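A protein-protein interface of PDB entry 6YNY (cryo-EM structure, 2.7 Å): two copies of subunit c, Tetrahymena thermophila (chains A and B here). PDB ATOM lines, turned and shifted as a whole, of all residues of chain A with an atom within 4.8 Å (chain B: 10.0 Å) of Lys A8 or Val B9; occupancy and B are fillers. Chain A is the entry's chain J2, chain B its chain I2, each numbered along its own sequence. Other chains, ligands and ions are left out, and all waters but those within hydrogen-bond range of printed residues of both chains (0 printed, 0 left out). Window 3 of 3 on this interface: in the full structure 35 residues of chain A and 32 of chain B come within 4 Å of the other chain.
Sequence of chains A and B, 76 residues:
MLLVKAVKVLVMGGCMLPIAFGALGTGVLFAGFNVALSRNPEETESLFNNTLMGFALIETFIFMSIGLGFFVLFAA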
ATOM      1  N   VAL A   4      28.449  -6.363 -17.218  1.00  0.00           N
ATOM      2  CA  VAL A   4      28.636  -5.883 -18.584  1.00  0.00           C
ATOM      3  C   VAL A   4      27.458  -6.299 -19.453  1.00  0.00           C
ATOM      4  O   VAL A   4      26.979  -5.525 -20.290  1.00  0.00           O
ATOM      5  CB  VAL A   4      29.971  -6.395 -19.155  1.00  0.00           C
ATOM      6  CG1 VAL A   4      30.080  -6.055 -20.620  1.00  0.00           C
ATOM      7  CG2 VAL A   4      31.135  -5.798 -18.391  1.00  0.00           C
ATOM      8  N   LYS A   5      26.970  -7.527 -19.268  1.00  0.00           N
ATOM      9  CA  LYS A   5      25.792  -7.968 -20.007  1.00  0.00           C
ATOM     10  C   LYS A   5      24.562  -7.171 -19.595  1.00  0.00           C
ATOM     11  O   LYS A   5      23.701  -6.869 -20.430  1.00  0.00           O
ATOM     12  CB  LYS A   5      25.564  -9.460 -19.777  1.00  0.00           C
ATOM     13  CG  LYS A   5      24.263  -9.999 -20.353  1.00  0.00           C
ATOM     14  CD  LYS A   5      24.157 -11.506 -20.154  1.00  0.00           C
ATOM     15  CE  LYS A   5      22.778 -12.029 -20.530  1.00  0.00           C
ATOM     16  NZ  LYS A   5      22.450 -11.815 -21.963  1.00  0.00           N
ATOM     17  N   ALA A   6      24.462  -6.828 -18.311  1.00  0.00           N
ATOM     18  CA  ALA A   6      23.294  -6.102 -17.827  1.00  0.00           C
ATOM     19  C   ALA A   6      23.248  -4.687 -18.390  1.00  0.00           C
ATOM     20  O   ALA A   6      22.178  -4.195 -18.766  1.00  0.00           O
ATOM     21  CB  ALA A   6      23.298  -6.078 -16.302  1.00  0.00           C
ATOM     22  N   VAL A   7      24.396  -4.008 -18.440  1.00  0.00           N
ATOM     23  CA  VAL A   7      24.425  -2.663 -19.004  1.00  0.00           C
ATOM     24  C   VAL A   7      24.179  -2.703 -20.505  1.00  0.00           C
ATOM     25  O   VAL A   7      23.611  -1.762 -21.074  1.00  0.00           O
ATOM     26  CB  VAL A   7      25.759  -1.970 -18.673  1.00  0.00           C
ATOM     27  CG1 VAL A   7      25.896  -1.783 -17.179  1.00  0.00           C
ATOM     28  CG2 VAL A   7      26.926  -2.768 -19.210  1.00  0.00           C
ATOM     29  N   LYS A   8      24.600  -3.777 -21.174  1.00  0.00           N
ATOM     30  CA  LYS A   8      24.332  -3.909 -22.602  1.00  0.00           C
ATOM     31  C   LYS A   8      22.835  -3.873 -22.879  1.00  0.00           C
ATOM     32  O   LYS A   8      22.362  -3.081 -23.702  1.00  0.00           O
ATOM     33  CB  LYS A   8      24.948  -5.203 -23.132  1.00  0.00           C
ATOM     34  CG  LYS A   8      26.407  -5.081 -23.544  1.00  0.00           C
ATOM     35  CD  LYS A   8      26.956  -6.424 -24.013  1.00  0.00           C
ATOM     36  CE  LYS A   8      28.295  -6.280 -24.722  1.00  0.00           C
ATOM     37  NZ  LYS A   8      29.379  -5.792 -23.824  1.00  0.00           N
ATOM     38  N   VAL A   9      22.070  -4.731 -22.199  1.00  0.00           N
ATOM     39  CA  VAL A   9      20.621  -4.720 -22.373  1.00  0.00           C
ATOM     40  C   VAL A   9      20.036  -3.393 -21.917  1.00  0.00           C
ATOM     41  O   VAL A   9      19.013  -2.942 -22.445  1.00  0.00           O
ATOM     42  CB  VAL A   9      19.979  -5.905 -21.624  1.00  0.00           C
ATOM     43  CG1 VAL A   9      20.341  -5.873 -20.156  1.00  0.00           C
ATOM     44  CG2 VAL A   9      18.474  -5.883 -21.794  1.00  0.00           C
ATOM     45  N   LEU A  10      20.665  -2.745 -20.935  1.00  0.00           N
ATOM     46  CA  LEU A  10      20.201  -1.429 -20.510  1.00  0.00           C
ATOM     47  C   LEU A  10      20.375  -0.410 -21.628  1.00  0.00           C
ATOM     48  O   LEU A  10      19.469   0.383 -21.908  1.00  0.00           O
ATOM     49  CB  LEU A  10      20.955  -0.985 -19.258  1.00  0.00           C
ATOM     50  CG  LEU A  10      20.529   0.363 -18.676  1.00  0.00           C
ATOM     51  CD1 LEU A  10      19.087   0.313 -18.201  1.00  0.00           C
ATOM     52  CD2 LEU A  10      21.455   0.773 -17.544  1.00  0.00           C
ATOM     53  N   VAL A  11      21.538  -0.418 -22.280  1.00  0.00           N
ATOM     54  CA  VAL A  11      21.760   0.468 -23.419  1.00  0.00           C
ATOM     55  C   VAL A  11      20.712   0.210 -24.492  1.00  0.00           C
ATOM     56  O   VAL A  11      20.111   1.140 -25.037  1.00  0.00           O
ATOM     57  CB  VAL A  11      23.186   0.294 -23.969  1.00  0.00           C
ATOM     58  CG1 VAL A  11      23.325   0.998 -25.307  1.00  0.00           C
ATOM     59  CG2 VAL A  11      24.206   0.823 -22.974  1.00  0.00           C
ATOM     60  N   MET A  12      20.470  -1.066 -24.800  1.00  0.00           N
ATOM     61  CA  MET A  12      19.477  -1.411 -25.811  1.00  0.00           C
ATOM     62  C   MET A  12      18.156  -0.698 -25.560  1.00  0.00           C
ATOM     63  O   MET A  12      17.432  -0.376 -26.509  1.00  0.00           O
ATOM     64  CB  MET A  12      19.268  -2.926 -25.836  1.00  0.00           C
ATOM     65  CG  MET A  12      18.330  -3.407 -26.921  1.00  0.00           C
ATOM     66  SD  MET A  12      18.896  -2.980 -28.575  1.00  0.00           S
ATOM     67  CE  MET A  12      17.637  -3.772 -29.563  1.00  0.00           C
ATOM     68  N   VAL A  72      25.571  -3.368 -30.041  1.00  0.00           N
ATOM     69  CA  VAL A  72      26.090  -3.331 -28.678  1.00  0.00           C
ATOM     70  C   VAL A  72      25.452  -4.424 -27.836  1.00  0.00           C
ATOM     71  O   VAL A  72      26.058  -4.914 -26.875  1.00  0.00           O
ATOM     72  CB  VAL A  72      25.863  -1.936 -28.064  1.00  0.00           C
ATOM     73  CG1 VAL A  72      26.372  -1.900 -26.646  1.00  0.00           C
ATOM     74  CG2 VAL A  72      26.549  -0.862 -28.898  1.00  0.00           C
ATOM     75  N   LEU A  73      24.227  -4.830 -28.179  1.00  0.00           N
ATOM     76  CA  LEU A  73      23.581  -5.933 -27.478  1.00  0.00           C
ATOM     77  C   LEU A  73      24.257  -7.264 -27.768  1.00  0.00           C
ATOM     78  O   LEU A  73      24.144  -8.193 -26.962  1.00  0.00           O
ATOM     79  CB  LEU A  73      22.105  -6.006 -27.875  1.00  0.00           C
ATOM     80  CG  LEU A  73      21.249  -7.065 -27.178  1.00  0.00           C
ATOM     81  CD1 LEU A  73      21.008  -6.684 -25.737  1.00  0.00           C
ATOM     82  CD2 LEU A  73      19.931  -7.261 -27.905  1.00  0.00           C
ATOM     83  N   ALA A  75      27.628  -7.174 -29.395  1.00  0.00           N
ATOM     84  CA  ALA A  75      29.040  -6.891 -29.630  1.00  0.00           C
ATOM     85  C   ALA A  75      29.573  -5.902 -28.601  1.00  0.00           C
ATOM     86  O   ALA A  75      28.813  -5.301 -27.842  1.00  0.00           O
ATOM     87  CB  ALA A  75      29.246  -6.353 -31.032  1.00  0.00           C
ATOM     88  N   MET B   1      39.117  -3.652 -15.362  1.00  0.00           N
ATOM     89  CA  MET B   1      38.916  -3.939 -16.812  1.00  0.00           C
ATOM     90  C   MET B   1      37.452  -4.251 -17.099  1.00  0.00           C
ATOM     91  O   MET B   1      36.761  -3.472 -17.758  1.00  0.00           O
ATOM     92  CB  MET B   1      39.808  -5.100 -17.267  1.00  0.00           C
ATOM     93  CG  MET B   1      40.174  -6.095 -16.171  1.00  0.00           C
ATOM     94  SD  MET B   1      41.160  -7.469 -16.799  1.00  0.00           S
ATOM     95  CE  MET B   1      41.607  -8.293 -15.274  1.00  0.00           C
ATOM     96  N   LEU B   2      36.978  -5.396 -16.603  1.00  0.00           N
ATOM     97  CA  LEU B   2      35.573  -5.745 -16.778  1.00  0.00           C
ATOM     98  C   LEU B   2      34.663  -4.723 -16.110  1.00  0.00           C
ATOM     99  O   LEU B   2      33.592  -4.398 -16.638  1.00  0.00           O
ATOM    100  CB  LEU B   2      35.305  -7.142 -16.219  1.00  0.00           C
ATOM    101  CG  LEU B   2      35.571  -8.314 -17.168  1.00  0.00           C
ATOM    102  CD1 LEU B   2      34.543  -8.336 -18.286  1.00  0.00           C
ATOM    103  CD2 LEU B   2      36.976  -8.249 -17.747  1.00  0.00           C
ATOM    104  N   LEU B   3      35.067  -4.203 -14.951  1.00  0.00           N
ATOM    105  CA  LEU B   3      34.267  -3.177 -14.294  1.00  0.00           C
ATOM    106  C   LEU B   3      34.208  -1.908 -15.134  1.00  0.00           C
ATOM    107  O   LEU B   3      33.128  -1.356 -15.374  1.00  0.00           O
ATOM    108  CB  LEU B   3      34.846  -2.882 -12.911  1.00  0.00           C
ATOM    109  CG  LEU B   3      34.190  -1.748 -12.121  1.00  0.00           C
ATOM    110  CD1 LEU B   3      32.690  -1.966 -11.976  1.00  0.00           C
ATOM    111  CD2 LEU B   3      34.855  -1.623 -10.762  1.00  0.00           C
ATOM    112  N   VAL B   4      35.365  -1.427 -15.595  1.00  0.00           N
ATOM    113  CA  VAL B   4      35.374  -0.233 -16.435  1.00  0.00           C
ATOM    114  C   VAL B   4      34.727  -0.519 -17.782  1.00  0.00           C
ATOM    115  O   VAL B   4      34.095   0.365 -18.374  1.00  0.00           O
ATOM    116  CB  VAL B   4      36.807   0.304 -16.596  1.00  0.00           C
ATOM    117  CG1 VAL B   4      36.893   1.230 -17.792  1.00  0.00           C
ATOM    118  CG2 VAL B   4      37.226   1.049 -15.343  1.00  0.00           C
ATOM    119  N   LYS B   5      34.876  -1.742 -18.299  1.00  0.00           N
ATOM    120  CA  LYS B   5      34.234  -2.081 -19.564  1.00  0.00           C
ATOM    121  C   LYS B   5      32.722  -1.938 -19.469  1.00  0.00           C
ATOM    122  O   LYS B   5      32.071  -1.557 -20.447  1.00  0.00           O
ATOM    123  CB  LYS B   5      34.605  -3.500 -19.990  1.00  0.00           C
ATOM    124  CG  LYS B   5      33.971  -3.916 -21.310  1.00  0.00           C
ATOM    125  CD  LYS B   5      34.482  -5.262 -21.790  1.00  0.00           C
ATOM    126  CE  LYS B   5      33.748  -5.710 -23.046  1.00  0.00           C
ATOM    127  NZ  LYS B   5      33.931  -4.754 -24.177  1.00  0.00           N
ATOM    128  N   ALA B   6      32.149  -2.244 -18.305  1.00  0.00           N
ATOM    129  CA  ALA B   6      30.707  -2.125 -18.134  1.00  0.00           C
ATOM    130  C   ALA B   6      30.248  -0.686 -18.327  1.00  0.00           C
ATOM    131  O   ALA B   6      29.231  -0.431 -18.980  1.00  0.00           O
ATOM    132  CB  ALA B   6      30.304  -2.640 -16.755  1.00  0.00           C
ATOM    133  N   VAL B   7      30.979   0.271 -17.752  1.00  0.00           N
ATOM    134  CA  VAL B   7      30.616   1.671 -17.932  1.00  0.00           C
ATOM    135  C   VAL B   7      31.013   2.154 -19.321  1.00  0.00           C
ATOM    136  O   VAL B   7      30.404   3.090 -19.853  1.00  0.00           O
ATOM    137  CB  VAL B   7      31.248   2.539 -16.830  1.00  0.00           C
ATOM    138  CG1 VAL B   7      30.677   2.161 -15.475  1.00  0.00           C
ATOM    139  CG2 VAL B   7      32.754   2.397 -16.824  1.00  0.00           C
ATOM    140  N   LYS B   8      32.031   1.541 -19.928  1.00  0.00           N
ATOM    141  CA  LYS B   8      32.377   1.866 -21.306  1.00  0.00           C
ATOM    142  C   LYS B   8      31.189   1.622 -22.228  1.00  0.00           C
ATOM    143  O   LYS B   8      30.746   2.521 -22.951  1.00  0.00           O
ATOM    144  CB  LYS B   8      33.577   1.031 -21.757  1.00  0.00           C
ATOM    145  CG  LYS B   8      34.942   1.635 -21.467  1.00  0.00           C
ATOM    146  CD  LYS B   8      36.049   0.706 -21.961  1.00  0.00           C
ATOM    147  CE  LYS B   8      37.401   1.401 -22.052  1.00  0.00           C
ATOM    148  NZ  LYS B   8      37.895   1.889 -20.738  1.00  0.00           N
ATOM    149  N   VAL B   9      30.656   0.397 -22.213  1.00  0.00           N
ATOM    150  CA  VAL B   9      29.512   0.076 -23.060  1.00  0.00           C
ATOM    151  C   VAL B   9      28.318   0.948 -22.707  1.00  0.00           C
ATOM    152  O   VAL B   9      27.529   1.319 -23.586  1.00  0.00           O
ATOM    153  CB  VAL B   9      29.166  -1.421 -22.945  1.00  0.00           C
ATOM    154  CG1 VAL B   9      28.902  -1.800 -21.507  1.00  0.00           C
ATOM    155  CG2 VAL B   9      27.955  -1.745 -23.789  1.00  0.00           C
ATOM    156  N   LEU B  10      28.157   1.289 -21.429  1.00  0.00           N
ATOM    157  CA  LEU B  10      27.065   2.173 -21.041  1.00  0.00           C
ATOM    158  C   LEU B  10      27.227   3.543 -21.684  1.00  0.00           C
ATOM    159  O   LEU B  10      26.259   4.118 -22.194  1.00  0.00           O
ATOM    160  CB  LEU B  10      26.999   2.297 -19.521  1.00  0.00           C
ATOM    161  CG  LEU B  10      25.798   3.076 -18.984  1.00  0.00           C
ATOM    162  CD1 LEU B  10      24.504   2.337 -19.273  1.00  0.00           C
ATOM    163  CD2 LEU B  10      25.949   3.326 -17.500  1.00  0.00           C
ATOM    164  N   VAL B  11      28.449   4.077 -21.670  1.00  0.00           N
ATOM    165  CA  VAL B  11      28.709   5.358 -22.319  1.00  0.00           C
ATOM    166  C   VAL B  11      28.393   5.268 -23.804  1.00  0.00           C
ATOM    167  O   VAL B  11      27.858   6.211 -24.399  1.00  0.00           O
ATOM    168  CB  VAL B  11      30.164   5.795 -22.075  1.00  0.00           C
ATOM    169  CG1 VAL B  11      30.552   6.901 -23.042  1.00  0.00           C
ATOM    170  CG2 VAL B  11      30.346   6.239 -20.630  1.00  0.00           C
ATOM    171  N   MET B  12      28.718   4.134 -24.430  1.00  0.00           N
ATOM    172  CA  MET B  12      28.396   3.963 -25.842  1.00  0.00           C
ATOM    173  C   MET B  12      26.902   4.118 -26.084  1.00  0.00           C
ATOM    174  O   MET B  12      26.490   4.568 -27.159  1.00  0.00           O
ATOM    175  CB  MET B  12      28.876   2.599 -26.336  1.00  0.00           C
ATOM    176  CG  MET B  12      28.663   2.380 -27.826  1.00  0.00           C
ATOM    177  SD  MET B  12      29.478   3.638 -28.826  1.00  0.00           S
ATOM    178  CE  MET B  12      28.786   3.290 -30.435  1.00  0.00           C
ATOM    179  N   GLY B  13      26.078   3.750 -25.103  1.00  0.00           N
ATOM    180  CA  GLY B  13      24.649   3.979 -25.224  1.00  0.00           C
ATOM    181  C   GLY B  13      24.304   5.453 -25.251  1.00  0.00           C
ATOM    182  O   GLY B  13      23.322   5.855 -25.882  1.00  0.00           O
ATOM    183  N   GLY B  14      25.101   6.278 -24.567  1.00  0.00           N
ATOM    184  CA  GLY B  14      24.852   7.708 -24.561  1.00  0.00           C
ATOM    185  C   GLY B  14      24.890   8.315 -25.948  1.00  0.00           C
ATOM    186  O   GLY B  14      24.239   9.330 -26.206  1.00  0.00           O
ATOM    187  N   CYS B  15      25.650   7.704 -26.859  1.00  0.00           N
ATOM    188  CA  CYS B  15      25.737   8.214 -28.220  1.00  0.00           C
ATOM    189  C   CYS B  15      24.385   8.224 -28.917  1.00  0.00           C
ATOM    190  O   CYS B  15      24.227   8.917 -29.928  1.00  0.00           O
ATOM    191  CB  CYS B  15      26.727   7.367 -29.020  1.00  0.00           C
ATOM    192  SG  CYS B  15      26.861   7.808 -30.764  1.00  0.00           S
ATOM    193  N   MET B  16      23.411   7.473 -28.410  1.00  0.00           N
ATOM    194  CA  MET B  16      22.072   7.469 -28.979  1.00  0.00           C
ATOM    195  C   MET B  16      21.267   8.704 -28.598  1.00  0.00           C
ATOM    196  O   MET B  16      20.110   8.820 -29.014  1.00  0.00           O
ATOM    197  CB  MET B  16      21.317   6.224 -28.520  1.00  0.00           C
ATOM    198  CG  MET B  16      21.927   4.923 -28.990  1.00  0.00           C
ATOM    199  SD  MET B  16      21.003   3.496 -28.399  1.00  0.00           S
ATOM    200  CE  MET B  16      21.162   3.714 -26.628  1.00  0.00           C
ATOM    201  N   GLY B  69      32.159   7.406 -29.593  1.00  0.00           N
ATOM    202  CA  GLY B  69      31.637   6.290 -28.829  1.00  0.00           C
ATOM    203  C   GLY B  69      32.512   5.057 -28.895  1.00  0.00           C
ATOM    204  O   GLY B  69      33.024   4.599 -27.869  1.00  0.00           O
ATOM    205  N   PHE B  70      32.686   4.500 -30.097  1.00  0.00           N
ATOM    206  CA  PHE B  70      33.529   3.319 -30.242  1.00  0.00           C
ATOM    207  C   PHE B  70      34.956   3.596 -29.792  1.00  0.00           C
ATOM    208  O   PHE B  70      35.652   2.682 -29.337  1.00  0.00           O
ATOM    209  CB  PHE B  70      33.526   2.834 -31.689  1.00  0.00           C
ATOM    210  CG  PHE B  70      32.243   2.179 -32.107  1.00  0.00           C
ATOM    211  CD1 PHE B  70      31.859   0.972 -31.554  1.00  0.00           C
ATOM    212  CD2 PHE B  70      31.431   2.761 -33.065  1.00  0.00           C
ATOM    213  CE1 PHE B  70      30.682   0.362 -31.935  1.00  0.00           C
ATOM    214  CE2 PHE B  70      30.251   2.151 -33.451  1.00  0.00           C
ATOM    215  CZ  PHE B  70      29.880   0.950 -32.886  1.00  0.00           C
ATOM    216  N   PHE B  71      35.412   4.841 -29.924  1.00  0.00           N
ATOM    217  CA  PHE B  71      36.765   5.184 -29.507  1.00  0.00           C
ATOM    218  C   PHE B  71      36.960   4.927 -28.019  1.00  0.00           C
ATOM    219  O   PHE B  71      37.773   4.086 -27.620  1.00  0.00           O
ATOM    220  CB  PHE B  71      37.056   6.645 -29.849  1.00  0.00           C
ATOM    221  CG  PHE B  71      38.440   7.086 -29.480  1.00  0.00           C
ATOM    222  CD1 PHE B  71      39.513   6.808 -30.312  1.00  0.00           C
ATOM    223  CD2 PHE B  71      38.671   7.784 -28.308  1.00  0.00           C
ATOM    224  CE1 PHE B  71      40.790   7.213 -29.978  1.00  0.00           C
ATOM    225  CE2 PHE B  71      39.944   8.191 -27.970  1.00  0.00           C
ATOM    226  CZ  PHE B  71      41.005   7.907 -28.805  1.00  0.00           C
ATOM    227  N   VAL B  72      36.219   5.649 -27.176  1.00  0.00           N
ATOM    228  CA  VAL B  72      36.326   5.438 -25.735  1.00  0.00           C
ATOM    229  C   VAL B  72      35.909   4.021 -25.370  1.00  0.00           C
ATOM    230  O   VAL B  72      36.347   3.481 -24.347  1.00  0.00           O
ATOM    231  CB  VAL B  72      35.490   6.487 -24.976  1.00  0.00           C
ATOM    232  CG1 VAL B  72      34.009   6.270 -25.224  1.00  0.00           C
ATOM    233  CG2 VAL B  72      35.804   6.439 -23.488  1.00  0.00           C
ATOM    234  N   LEU B  73      35.068   3.394 -26.194  1.00  0.00           N
ATOM    235  CA  LEU B  73      34.691   2.007 -25.955  1.00  0.00           C
ATOM    236  C   LEU B  73      35.889   1.074 -26.049  1.00  0.00           C
ATOM    237  O   LEU B  73      35.838  -0.041 -25.518  1.00  0.00           O
ATOM    238  CB  LEU B  73      33.610   1.586 -26.951  1.00  0.00           C
ATOM    239  CG  LEU B  73      33.134   0.134 -26.913  1.00  0.00           C
ATOM    240  CD1 LEU B  73      32.603  -0.236 -25.550  1.00  0.00           C
ATOM    241  CD2 LEU B  73      32.061  -0.083 -27.966  1.00  0.00           C
ATOM    242  N   PHE B  74      36.961   1.507 -26.712  1.00  0.00           N
ATOM    243  CA  PHE B  74      38.164   0.705 -26.864  1.00  0.00           C
ATOM    244  C   PHE B  74      39.436   1.443 -26.470  1.00  0.00           C
ATOM    245  O   PHE B  74      40.472   0.791 -26.299  1.00  0.00           O
ATOM    246  CB  PHE B  74      38.297   0.213 -28.313  1.00  0.00           C
ATOM    247  CG  PHE B  74      37.134  -0.621 -28.778  1.00  0.00           C
ATOM    248  CD1 PHE B  74      36.580  -1.586 -27.952  1.00  0.00           C
ATOM    249  CD2 PHE B  74      36.590  -0.435 -30.036  1.00  0.00           C
ATOM    250  CE1 PHE B  74      35.511  -2.353 -28.375  1.00  0.00           C
ATOM    251  CE2 PHE B  74      35.519  -1.198 -30.463  1.00  0.00           C
ATOM    252  CZ  PHE B  74      34.980  -2.156 -29.631  1.00  0.00           C
ATOM    253  N   ALA B  75      39.393   2.764 -26.318  1.00  0.00           N
ATOM    254  CA  ALA B  75      40.559   3.542 -25.914  1.00  0.00           C
ATOM    255  C   ALA B  75      40.430   3.983 -24.461  1.00  0.00           C
ATOM    256  O   ALA B  75      39.368   3.854 -23.854  1.00  0.00           O
ATOM    257  CB  ALA B  75      40.730   4.750 -26.814  1.00  0.00           C
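Val A4 touches Ala B6. Val A7 touches Ala B6 (CG2 to O, 3.3 Å). CG2 of Val A7 touches CG1 of Val B9, 3.2 Å away. CG of Lys A8 touches CG2 of Val B9, at 3.7 Å. Leu A10 touches Leu B10 (CD2 to CD1, 3.8 Å). Val B9 touches Val A11. Leu B10 touches Val A11 (CA to CG2, 3.7 Å). CG1 of Val A11 touches CA of Gly B13, at 3.3 Å. O of Val A11 touches CE of Met B16 (3.2 Å). Val B9 touches Val A72 (CG2 to CG1, 3.3 Å).
Of chain B, only Val B9 comes within 4 Å of Lys A8. Val B9 touches just these residues of chain A: Val A7 (3.2 Å), Lys A8 (3.7 Å), Val A11 (3.4 Å) and Val A72 (3.3 Å). No residue of chain B comes within 4 Å of Ala A6. Val A7 touches just these residues of chain B: Ala B6 and Val B9. No residue of chain B comes within 4 Å of Val A9. Val A11 touches four residues of chain B. Printed residues of chain A within 4 Å of Leu B10: Leu A10 and Val A11. Printed residues of chain A within 4 Å of Gly B13: Val A11. Ala A75 touches none of the printed residues of chain B. The nearest residue of chain B that does not touch Lys A8 is Lys B5 (4.4 Å).
Hydrophobic or aromatic side chains of chain A that line the printed part of chain B: Val A4, Val A7, Leu A10, Val A11 and Val A72. Hydrophobic or aromatic side chains of chain B that line the printed part of chain A: Ala B6, Val B9, Leu B10 and Met B16. Among the printed residues, 11 pairs touch across the chains. Among the printed residues, no Asp or Glu carboxylate lies within 4 Å of a Lys or Arg side-chain nitrogen of the other chain.
Val A4 touches Ala B6, but with the chains exchanged Ala A6 does not touch Val B4 (12.0 Å). Val A7 touches Val B9, but with the chains exchanged Val A9 does not touch Val B7 (11.1 Å). Lys A8 touches Val B9, but with the chains exchanged Val A9 does not touch Lys B8 (11.1 Å). Val A11 touches Val B9, but with the chains exchanged Val A9 does not touch Val B11 (10.9 Å).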
